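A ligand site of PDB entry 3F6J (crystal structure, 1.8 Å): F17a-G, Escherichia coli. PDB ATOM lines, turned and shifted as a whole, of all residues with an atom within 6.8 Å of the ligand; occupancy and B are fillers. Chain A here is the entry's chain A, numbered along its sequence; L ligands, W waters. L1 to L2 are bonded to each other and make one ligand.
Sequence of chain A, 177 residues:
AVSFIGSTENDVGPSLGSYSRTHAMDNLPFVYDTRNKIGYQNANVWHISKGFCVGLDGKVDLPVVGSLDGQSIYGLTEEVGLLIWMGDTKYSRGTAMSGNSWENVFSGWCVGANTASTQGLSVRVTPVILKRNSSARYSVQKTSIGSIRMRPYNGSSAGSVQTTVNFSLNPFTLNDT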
ATOM      1  N   ASN A  42      20.613   2.171 -13.656  1.00  0.00           N
ATOM      2  CA  ASN A  42      20.045   3.500 -13.343  1.00  0.00           C
ATOM      3  C   ASN A  42      21.173   4.523 -13.331  1.00  0.00           C
ATOM      4  O   ASN A  42      22.086   4.400 -12.505  1.00  0.00           O
ATOM      5  CB  ASN A  42      19.338   3.466 -11.977  1.00  0.00           C
ATOM      6  CG  ASN A  42      18.517   4.734 -11.692  1.00  0.00           C
ATOM      7  OD1 ASN A  42      18.740   5.763 -12.311  1.00  0.00           O
ATOM      8  ND2 ASN A  42      17.574   4.646 -10.733  1.00  0.00           N
ATOM      9  N   ALA A  43      21.136   5.477 -14.275  1.00  0.00           N
ATOM     10  CA  ALA A  43      22.159   6.531 -14.374  1.00  0.00           C
ATOM     11  C   ALA A  43      22.094   7.504 -13.203  1.00  0.00           C
ATOM     12  O   ALA A  43      23.073   8.207 -12.938  1.00  0.00           O
ATOM     13  CB  ALA A  43      22.040   7.320 -15.715  1.00  0.00           C
ATOM     14  N   ASN A  44      20.952   7.537 -12.509  1.00  0.00           N
ATOM     15  CA  ASN A  44      20.634   8.631 -11.569  1.00  0.00           C
ATOM     16  C   ASN A  44      20.199   8.132 -10.177  1.00  0.00           C
ATOM     17  O   ASN A  44      19.017   8.242  -9.799  1.00  0.00           O
ATOM     18  CB  ASN A  44      19.549   9.501 -12.190  1.00  0.00           C
ATOM     19  CG  ASN A  44      19.891   9.937 -13.619  1.00  0.00           C
ATOM     20  OD1 ASN A  44      19.190   9.605 -14.587  1.00  0.00           O
ATOM     21  ND2 ASN A  44      20.955  10.675 -13.742  1.00  0.00           N
ATOM     22  N   VAL A  45      21.161   7.611  -9.416  1.00  0.00           N
ATOM     23  CA  VAL A  45      20.847   7.024  -8.115  1.00  0.00           C
ATOM     24  C   VAL A  45      21.150   8.020  -6.969  1.00  0.00           C
ATOM     25  O   VAL A  45      20.361   8.133  -6.027  1.00  0.00           O
ATOM     26  CB  VAL A  45      21.561   5.656  -7.917  1.00  0.00           C
ATOM     27  CG1 VAL A  45      21.272   5.087  -6.516  1.00  0.00           C
ATOM     28  CG2 VAL A  45      21.109   4.657  -9.004  1.00  0.00           C
ATOM     29  N   ILE A  48      24.745  14.604  -7.143  1.00  0.00           N
ATOM     30  CA  ILE A  48      26.002  15.099  -6.538  1.00  0.00           C
ATOM     31  C   ILE A  48      26.395  16.447  -7.143  1.00  0.00           C
ATOM     32  O   ILE A  48      26.083  16.744  -8.299  1.00  0.00           O
ATOM     33  CB  ILE A  48      27.195  14.091  -6.653  1.00  0.00           C
ATOM     34  CG1 ILE A  48      27.553  13.760  -8.113  1.00  0.00           C
ATOM     35  CG2 ILE A  48      26.937  12.828  -5.810  1.00  0.00           C
ATOM     36  CD1 ILE A  48      28.844  12.881  -8.253  1.00  0.00           C
ATOM     37  N   VAL A  54      33.014  10.429  -5.450  1.00  0.00           N
ATOM     38  CA  VAL A  54      32.280   9.208  -5.087  1.00  0.00           C
ATOM     39  C   VAL A  54      32.585   8.037  -6.018  1.00  0.00           C
ATOM     40  O   VAL A  54      32.658   8.196  -7.249  1.00  0.00           O
ATOM     41  CB  VAL A  54      30.755   9.485  -5.010  1.00  0.00           C
ATOM     42  CG1 VAL A  54      30.171   9.782  -6.386  1.00  0.00           C
ATOM     43  CG2 VAL A  54      30.034   8.340  -4.315  1.00  0.00           C
ATOM     44  N   LEU A  56      31.892   3.344  -5.931  1.00  0.00           N
ATOM     45  CA  LEU A  56      30.889   2.347  -5.521  1.00  0.00           C
ATOM     46  C   LEU A  56      31.540   1.085  -4.952  1.00  0.00           C
ATOM     47  O   LEU A  56      32.510   0.596  -5.540  1.00  0.00           O
ATOM     48  CB  LEU A  56      30.020   1.906  -6.705  1.00  0.00           C
ATOM     49  CG  LEU A  56      29.179   2.941  -7.463  1.00  0.00           C
ATOM     50  CD1 LEU A  56      28.572   2.243  -8.683  1.00  0.00           C
ATOM     51  CD2 LEU A  56      28.095   3.526  -6.550  1.00  0.00           C
ATOM     52  N   ASP A  88      29.592   0.928 -12.129  1.00  0.00           N
ATOM     53  CA  ASP A  88      29.049   2.179 -12.666  1.00  0.00           C
ATOM     54  C   ASP A  88      27.913   1.929 -13.681  1.00  0.00           C
ATOM     55  O   ASP A  88      27.680   0.798 -14.118  1.00  0.00           O
ATOM     56  CB  ASP A  88      30.179   2.988 -13.310  1.00  0.00           C
ATOM     57  CG  ASP A  88      29.852   4.463 -13.466  1.00  0.00           C
ATOM     58  OD1 ASP A  88      29.048   5.007 -12.672  1.00  0.00           O
ATOM     59  OD2 ASP A  88      30.424   5.078 -14.388  1.00  0.00           O
ATOM     60  N   THR A  89      27.236   3.002 -14.067  1.00  0.00           N
ATOM     61  CA  THR A  89      26.082   2.952 -14.949  1.00  0.00           C
ATOM     62  C   THR A  89      26.189   2.041 -16.176  1.00  0.00           C
ATOM     63  O   THR A  89      25.360   1.147 -16.355  1.00  0.00           O
ATOM     64  CB  THR A  89      25.696   4.378 -15.387  1.00  0.00           C
ATOM     65  OG1 THR A  89      25.570   5.192 -14.212  1.00  0.00           O
ATOM     66  CG2 THR A  89      24.390   4.395 -16.197  1.00  0.00           C
ATOM     67  N   LYS A  90      27.175   2.297 -17.043  1.00  0.00           N
ATOM     68  CA  LYS A  90      27.291   1.517 -18.283  1.00  0.00           C
ATOM     69  C   LYS A  90      27.627   0.053 -18.004  1.00  0.00           C
ATOM     70  O   LYS A  90      28.555  -0.247 -17.244  1.00  0.00           O
ATOM     71  CB  LYS A  90      28.388   2.084 -19.194  1.00  0.00           C
ATOM     72  CG  LYS A  90      28.290   3.540 -19.427  1.00  0.00           C
ATOM     73  CD  LYS A  90      27.389   3.835 -20.565  1.00  0.00           C
ATOM     74  CE  LYS A  90      27.661   5.222 -21.043  1.00  0.00           C
ATOM     75  NZ  LYS A  90      26.375   5.857 -21.278  1.00  0.00           N
ATOM     76  N   PHE A 106      33.638   0.356  -8.561  1.00  0.00           N
ATOM     77  CA  PHE A 106      33.823   1.572  -9.371  1.00  0.00           C
ATOM     78  C   PHE A 106      34.786   2.478  -8.585  1.00  0.00           C
ATOM     79  O   PHE A 106      34.431   2.953  -7.522  1.00  0.00           O
ATOM     80  CB  PHE A 106      32.480   2.294  -9.666  1.00  0.00           C
ATOM     81  CG  PHE A 106      32.663   3.637 -10.348  1.00  0.00           C
ATOM     82  CD1 PHE A 106      33.572   3.780 -11.390  1.00  0.00           C
ATOM     83  CD2 PHE A 106      31.930   4.747  -9.935  1.00  0.00           C
ATOM     84  CE1 PHE A 106      33.758   5.017 -12.008  1.00  0.00           C
ATOM     85  CE2 PHE A 106      32.103   5.980 -10.555  1.00  0.00           C
ATOM     86  CZ  PHE A 106      33.014   6.109 -11.582  1.00  0.00           C
ATOM     87  N   GLY A 108      35.714   5.451  -8.937  1.00  0.00           N
ATOM     88  CA  GLY A 108      35.127   6.751  -8.594  1.00  0.00           C
ATOM     89  C   GLY A 108      35.436   7.906  -9.509  1.00  0.00           C
ATOM     90  O   GLY A 108      36.266   7.828 -10.421  1.00  0.00           O
ATOM     91  N   TRP A 109      34.705   8.994  -9.304  1.00  0.00           N
ATOM     92  CA  TRP A 109      35.003  10.244  -9.994  1.00  0.00           C
ATOM     93  C   TRP A 109      34.580  11.406  -9.099  1.00  0.00           C
ATOM     94  O   TRP A 109      33.933  11.190  -8.051  1.00  0.00           O
ATOM     95  CB  TRP A 109      34.271  10.309 -11.342  1.00  0.00           C
ATOM     96  CG  TRP A 109      32.806  10.556 -11.217  1.00  0.00           C
ATOM     97  CD1 TRP A 109      31.861   9.740 -10.604  1.00  0.00           C
ATOM     98  CD2 TRP A 109      32.087  11.673 -11.738  1.00  0.00           C
ATOM     99  NE1 TRP A 109      30.615  10.314 -10.719  1.00  0.00           N
ATOM    100  CE2 TRP A 109      30.724  11.495 -11.398  1.00  0.00           C
ATOM    101  CE3 TRP A 109      32.478  12.832 -12.433  1.00  0.00           C
ATOM    102  CZ2 TRP A 109      29.738  12.436 -11.748  1.00  0.00           C
ATOM    103  CZ3 TRP A 109      31.502  13.755 -12.773  1.00  0.00           C
ATOM    104  CH2 TRP A 109      30.159  13.554 -12.445  1.00  0.00           C
ATOM    105  N   CYS A 110      34.957  12.615  -9.514  1.00  0.00           N
ATOM    106  CA  CYS A 110      34.590  13.858  -8.801  1.00  0.00           C
ATOM    107  C   CYS A 110      33.845  14.797  -9.740  1.00  0.00           C
ATOM    108  O   CYS A 110      34.370  15.181 -10.803  1.00  0.00           O
ATOM    109  CB  CYS A 110      35.827  14.571  -8.260  1.00  0.00           C
ATOM    110  SG  CYS A 110      36.852  13.566  -7.197  1.00  0.00           S
ATOM    111  N   VAL A 111      32.634  15.167  -9.339  1.00  0.00           N
ATOM    112  CA  VAL A 111      31.859  16.142 -10.109  1.00  0.00           C
ATOM    113  C   VAL A 111      32.541  17.525 -10.033  1.00  0.00           C
ATOM    114  O   VAL A 111      33.227  17.813  -9.036  1.00  0.00           O
ATOM    115  CB  VAL A 111      30.388  16.191  -9.598  1.00  0.00           C
ATOM    116  CG1 VAL A 111      30.350  16.733  -8.167  1.00  0.00           C
ATOM    117  CG2 VAL A 111      29.506  16.994 -10.556  1.00  0.00           C
ATOM    118  N   THR A 115      29.633  22.614 -10.436  1.00  0.00           N
ATOM    119  CA  THR A 115      28.550  22.038 -11.244  1.00  0.00           C
ATOM    120  C   THR A 115      27.878  20.869 -10.552  1.00  0.00           C
ATOM    121  O   THR A 115      28.220  20.539  -9.405  1.00  0.00           O
ATOM    122  CB  THR A 115      29.070  21.637 -12.639  1.00  0.00           C
ATOM    123  OG1 THR A 115      30.087  20.633 -12.499  1.00  0.00           O
ATOM    124  CG2 THR A 115      29.656  22.847 -13.365  1.00  0.00           C
ATOM    125  N   ALA A 116      26.896  20.274 -11.221  1.00  0.00           N
ATOM    126  CA  ALA A 116      26.139  19.143 -10.650  1.00  0.00           C
ATOM    127  C   ALA A 116      26.004  18.022 -11.659  1.00  0.00           C
ATOM    128  O   ALA A 116      26.076  18.250 -12.877  1.00  0.00           O
ATOM    129  CB  ALA A 116      24.773  19.596 -10.174  1.00  0.00           C
ATOM    130  N   SER A 117      25.794  16.805 -11.145  1.00  0.00           N
ATOM    131  CA  SER A 117      25.572  15.644 -11.970  1.00  0.00           C
ATOM    132  C   SER A 117      24.928  14.575 -11.095  1.00  0.00           C
ATOM    133  O   SER A 117      24.309  14.873 -10.061  1.00  0.00           O
ATOM    134  CB  SER A 117      26.880  15.150 -12.594  1.00  0.00           C
ATOM    135  OG  SER A 117      26.632  14.181 -13.591  1.00  0.00           O
ATOM    136  N   THR A 118      25.061  13.322 -11.518  1.00  0.00           N
ATOM    137  CA  THR A 118      24.537  12.216 -10.753  1.00  0.00           C
ATOM    138  C   THR A 118      25.554  11.094 -10.731  1.00  0.00           C
ATOM    139  O   THR A 118      26.479  11.050 -11.578  1.00  0.00           O
ATOM    140  CB  THR A 118      23.235  11.643 -11.387  1.00  0.00           C
ATOM    141  OG1 THR A 118      23.539  11.203 -12.708  1.00  0.00           O
ATOM    142  CG2 THR A 118      22.087  12.690 -11.396  1.00  0.00           C
ATOM    143  N   GLN A 119      25.373  10.175  -9.794  1.00  0.00           N
ATOM    144  CA  GLN A 119      26.109   8.909  -9.766  1.00  0.00           C
ATOM    145  C   GLN A 119      25.103   7.759  -9.951  1.00  0.00           C
ATOM    146  O   GLN A 119      24.085   7.678  -9.232  1.00  0.00           O
ATOM    147  CB  GLN A 119      26.866   8.760  -8.420  1.00  0.00           C
ATOM    148  CG  GLN A 119      27.554   7.384  -8.241  1.00  0.00           C
ATOM    149  CD  GLN A 119      28.589   7.129  -9.315  1.00  0.00           C
ATOM    150  OE1 GLN A 119      29.358   8.034  -9.645  1.00  0.00           O
ATOM    151  NE2 GLN A 119      28.590   5.910  -9.898  1.00  0.00           N
ATOM    152  N   GLY A 120      25.364   6.875 -10.930  1.00  0.00           N
ATOM    153  CA  GLY A 120      24.480   5.752 -11.245  1.00  0.00           C
ATOM    154  C   GLY A 120      25.104   4.413 -10.920  1.00  0.00           C
ATOM    155  O   GLY A 120      26.178   4.334 -10.299  1.00  0.00           O
ATOM    156  N   LEU A 121      24.433   3.344 -11.324  1.00  0.00           N
ATOM    157  CA  LEU A 121      25.003   2.002 -11.123  1.00  0.00           C
ATOM    158  C   LEU A 121      24.388   1.003 -12.089  1.00  0.00           C
ATOM    159  O   LEU A 121      23.383   1.287 -12.755  1.00  0.00           O
ATOM    160  CB  LEU A 121      24.825   1.567  -9.658  1.00  0.00           C
ATOM    161  CG  LEU A 121      23.393   1.616  -9.095  1.00  0.00           C
ATOM    162  CD1 LEU A 121      22.490   0.480  -9.663  1.00  0.00           C
ATOM    163  CD2 LEU A 121      23.366   1.662  -7.565  1.00  0.00           C
HETATM  164  C1  LIG L   1      29.705  14.825 -16.717  1.00  0.00           C
HETATM  165  C2  LIG L   1      28.568  13.807 -16.567  1.00  0.00           C
HETATM  166  C3  LIG L   1      29.048  12.581 -15.782  1.00  0.00           C
HETATM  167  C4  LIG L   1      30.425  12.011 -16.263  1.00  0.00           C
HETATM  168  C5  LIG L   1      31.437  13.150 -16.446  1.00  0.00           C
HETATM  169  C6  LIG L   1      32.767  12.741 -17.115  1.00  0.00           C
HETATM  170  C7  LIG L   1      30.288  17.000 -17.468  1.00  0.00           C
HETATM  171  O1  LIG L   1      29.326  15.911 -17.569  1.00  0.00           O
HETATM  172  O2  LIG L   1      27.447  14.417 -15.879  1.00  0.00           O
HETATM  173  O3  LIG L   1      27.946  11.662 -15.936  1.00  0.00           O
HETATM  174  O4  LIG L   1      30.220  11.304 -17.488  1.00  0.00           O
HETATM  175  O5  LIG L   1      30.868  14.174 -17.294  1.00  0.00           O
HETATM  176  O6  LIG L   1      33.624  13.891 -17.054  1.00  0.00           O
HETATM  177  C1  LG2 L   2      27.762  10.805 -14.780  1.00  0.00           C
HETATM  178  C2  LG2 L   2      26.487   9.925 -14.972  1.00  0.00           C
HETATM  179  C3  LG2 L   2      26.342   8.796 -13.923  1.00  0.00           C
HETATM  180  C4  LG2 L   2      27.679   8.031 -13.699  1.00  0.00           C
HETATM  181  C5  LG2 L   2      28.821   9.047 -13.495  1.00  0.00           C
HETATM  182  C6  LG2 L   2      30.197   8.409 -13.291  1.00  0.00           C
HETATM  183  C7  LG2 L   2      24.585  11.030 -16.049  1.00  0.00           C
HETATM  184  C8  LG2 L   2      25.063  10.341 -17.330  1.00  0.00           C
HETATM  185  N1  LG2 L   2      25.284  10.778 -14.941  1.00  0.00           N
HETATM  186  O1  LG2 L   2      25.290   7.946 -14.399  1.00  0.00           O
HETATM  187  O2  LG2 L   2      27.601   7.134 -12.582  1.00  0.00           O
HETATM  188  O3  LG2 L   2      28.899   9.930 -14.668  1.00  0.00           O
HETATM  189  O4  LG2 L   2      30.564   7.772 -14.505  1.00  0.00           O
HETATM  190  O5  LG2 L   2      23.588  11.750 -16.050  1.00  0.00           O
HETATM  191  O   HOH W   1      32.974  16.295 -15.224  1.00  0.00           O
HETATM  192  O   HOH W   2      35.928  12.856 -18.108  1.00  0.00           O
HETATM  193  O   HOH W   3      25.395   7.402 -17.520  1.00  0.00           O
HETATM  194  O   HOH W   4      30.214   8.489 -17.026  1.00  0.00           O
HETATM  195  O   HOH W   5      26.194  16.478 -17.190  1.00  0.00           O
HETATM  196  O   HOH W   6      22.529   9.925 -18.627  1.00  0.00           O
HETATM  197  O   HOH W   7      32.187  15.078 -19.674  1.00  0.00           O
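The side-chain carboxylate (OD1) of Asp 88 lies within hydrogen-bond range of the side-chain amide nitrogen (NE2) of Gln 119, 3.0 Å away.
The backbone NH (N) of Gly 120 sits close to the backbone carbonyl oxygen (O) of Ala 43, at 3.3 Å.
The backbone carbonyl oxygen (O) of Ala 43 is in hydrogen-bond range of the side-chain hydroxyl (OG1) of Thr 118 (3.0 Å).
The side-chain hydroxyl of Thr 118 lies within hydrogen-bond range of the side-chain amide nitrogen of Asn 44.
The side-chain amide oxygen (OE1) of Gln 119 sits at hydrogen-bond distance from the indole nitrogen (NE1) of Trp 109 (2.8 Å).
The backbone NH (N) of Val 45 lies within hydrogen-bond range of the backbone carbonyl oxygen (O) of Gln 119 (2.9 Å).
The backbone NH (N) of Val 54 sits at hydrogen-bond distance from the backbone carbonyl oxygen (O) of Trp 109.
N of Asn 44 lies within hydrogen-bond range of OD1 of Asn 42.
Asn 44 touches the ligand.
Trp 109 touches the ligand.
Hydrophobic or aromatic side chains within 4 Å of the ligand: Ala 43 and Trp 109.
Within 4 Å of the ligand: Ala 43, Asn 44, Asp 88, Thr 89, Trp 109, Ser 117, Thr 118, Gln 119 and Gly 120.
The side-chain hydroxyl (OG) of Ser 117 sits at hydrogen-bond distance from an oxygen (O2) of LIG L1, 2.4 Å away.
The side-chain carboxylate of Asp 88 sits at hydrogen-bond distance from an oxygen (O2) of LG2 L2 (2.6 Å).
O of Ala 43 sits at hydrogen-bond distance from O1 of LG2 L2 (2.7 Å).
O1 of LG2 L2 lies within hydrogen-bond range of OG1 of Thr 89 (2.8 Å).
The backbone NH (N) of Gly 120 is in hydrogen-bond range of an oxygen (O2) of LG2 L2 (2.8 Å).
OG1 of Thr 118 lies within hydrogen-bond range of N1 of LG2 L2 (2.9 Å).
The side-chain amide nitrogen (NE2) of Gln 119 sits at hydrogen-bond distance from an oxygen (O2) of LG2 L2.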
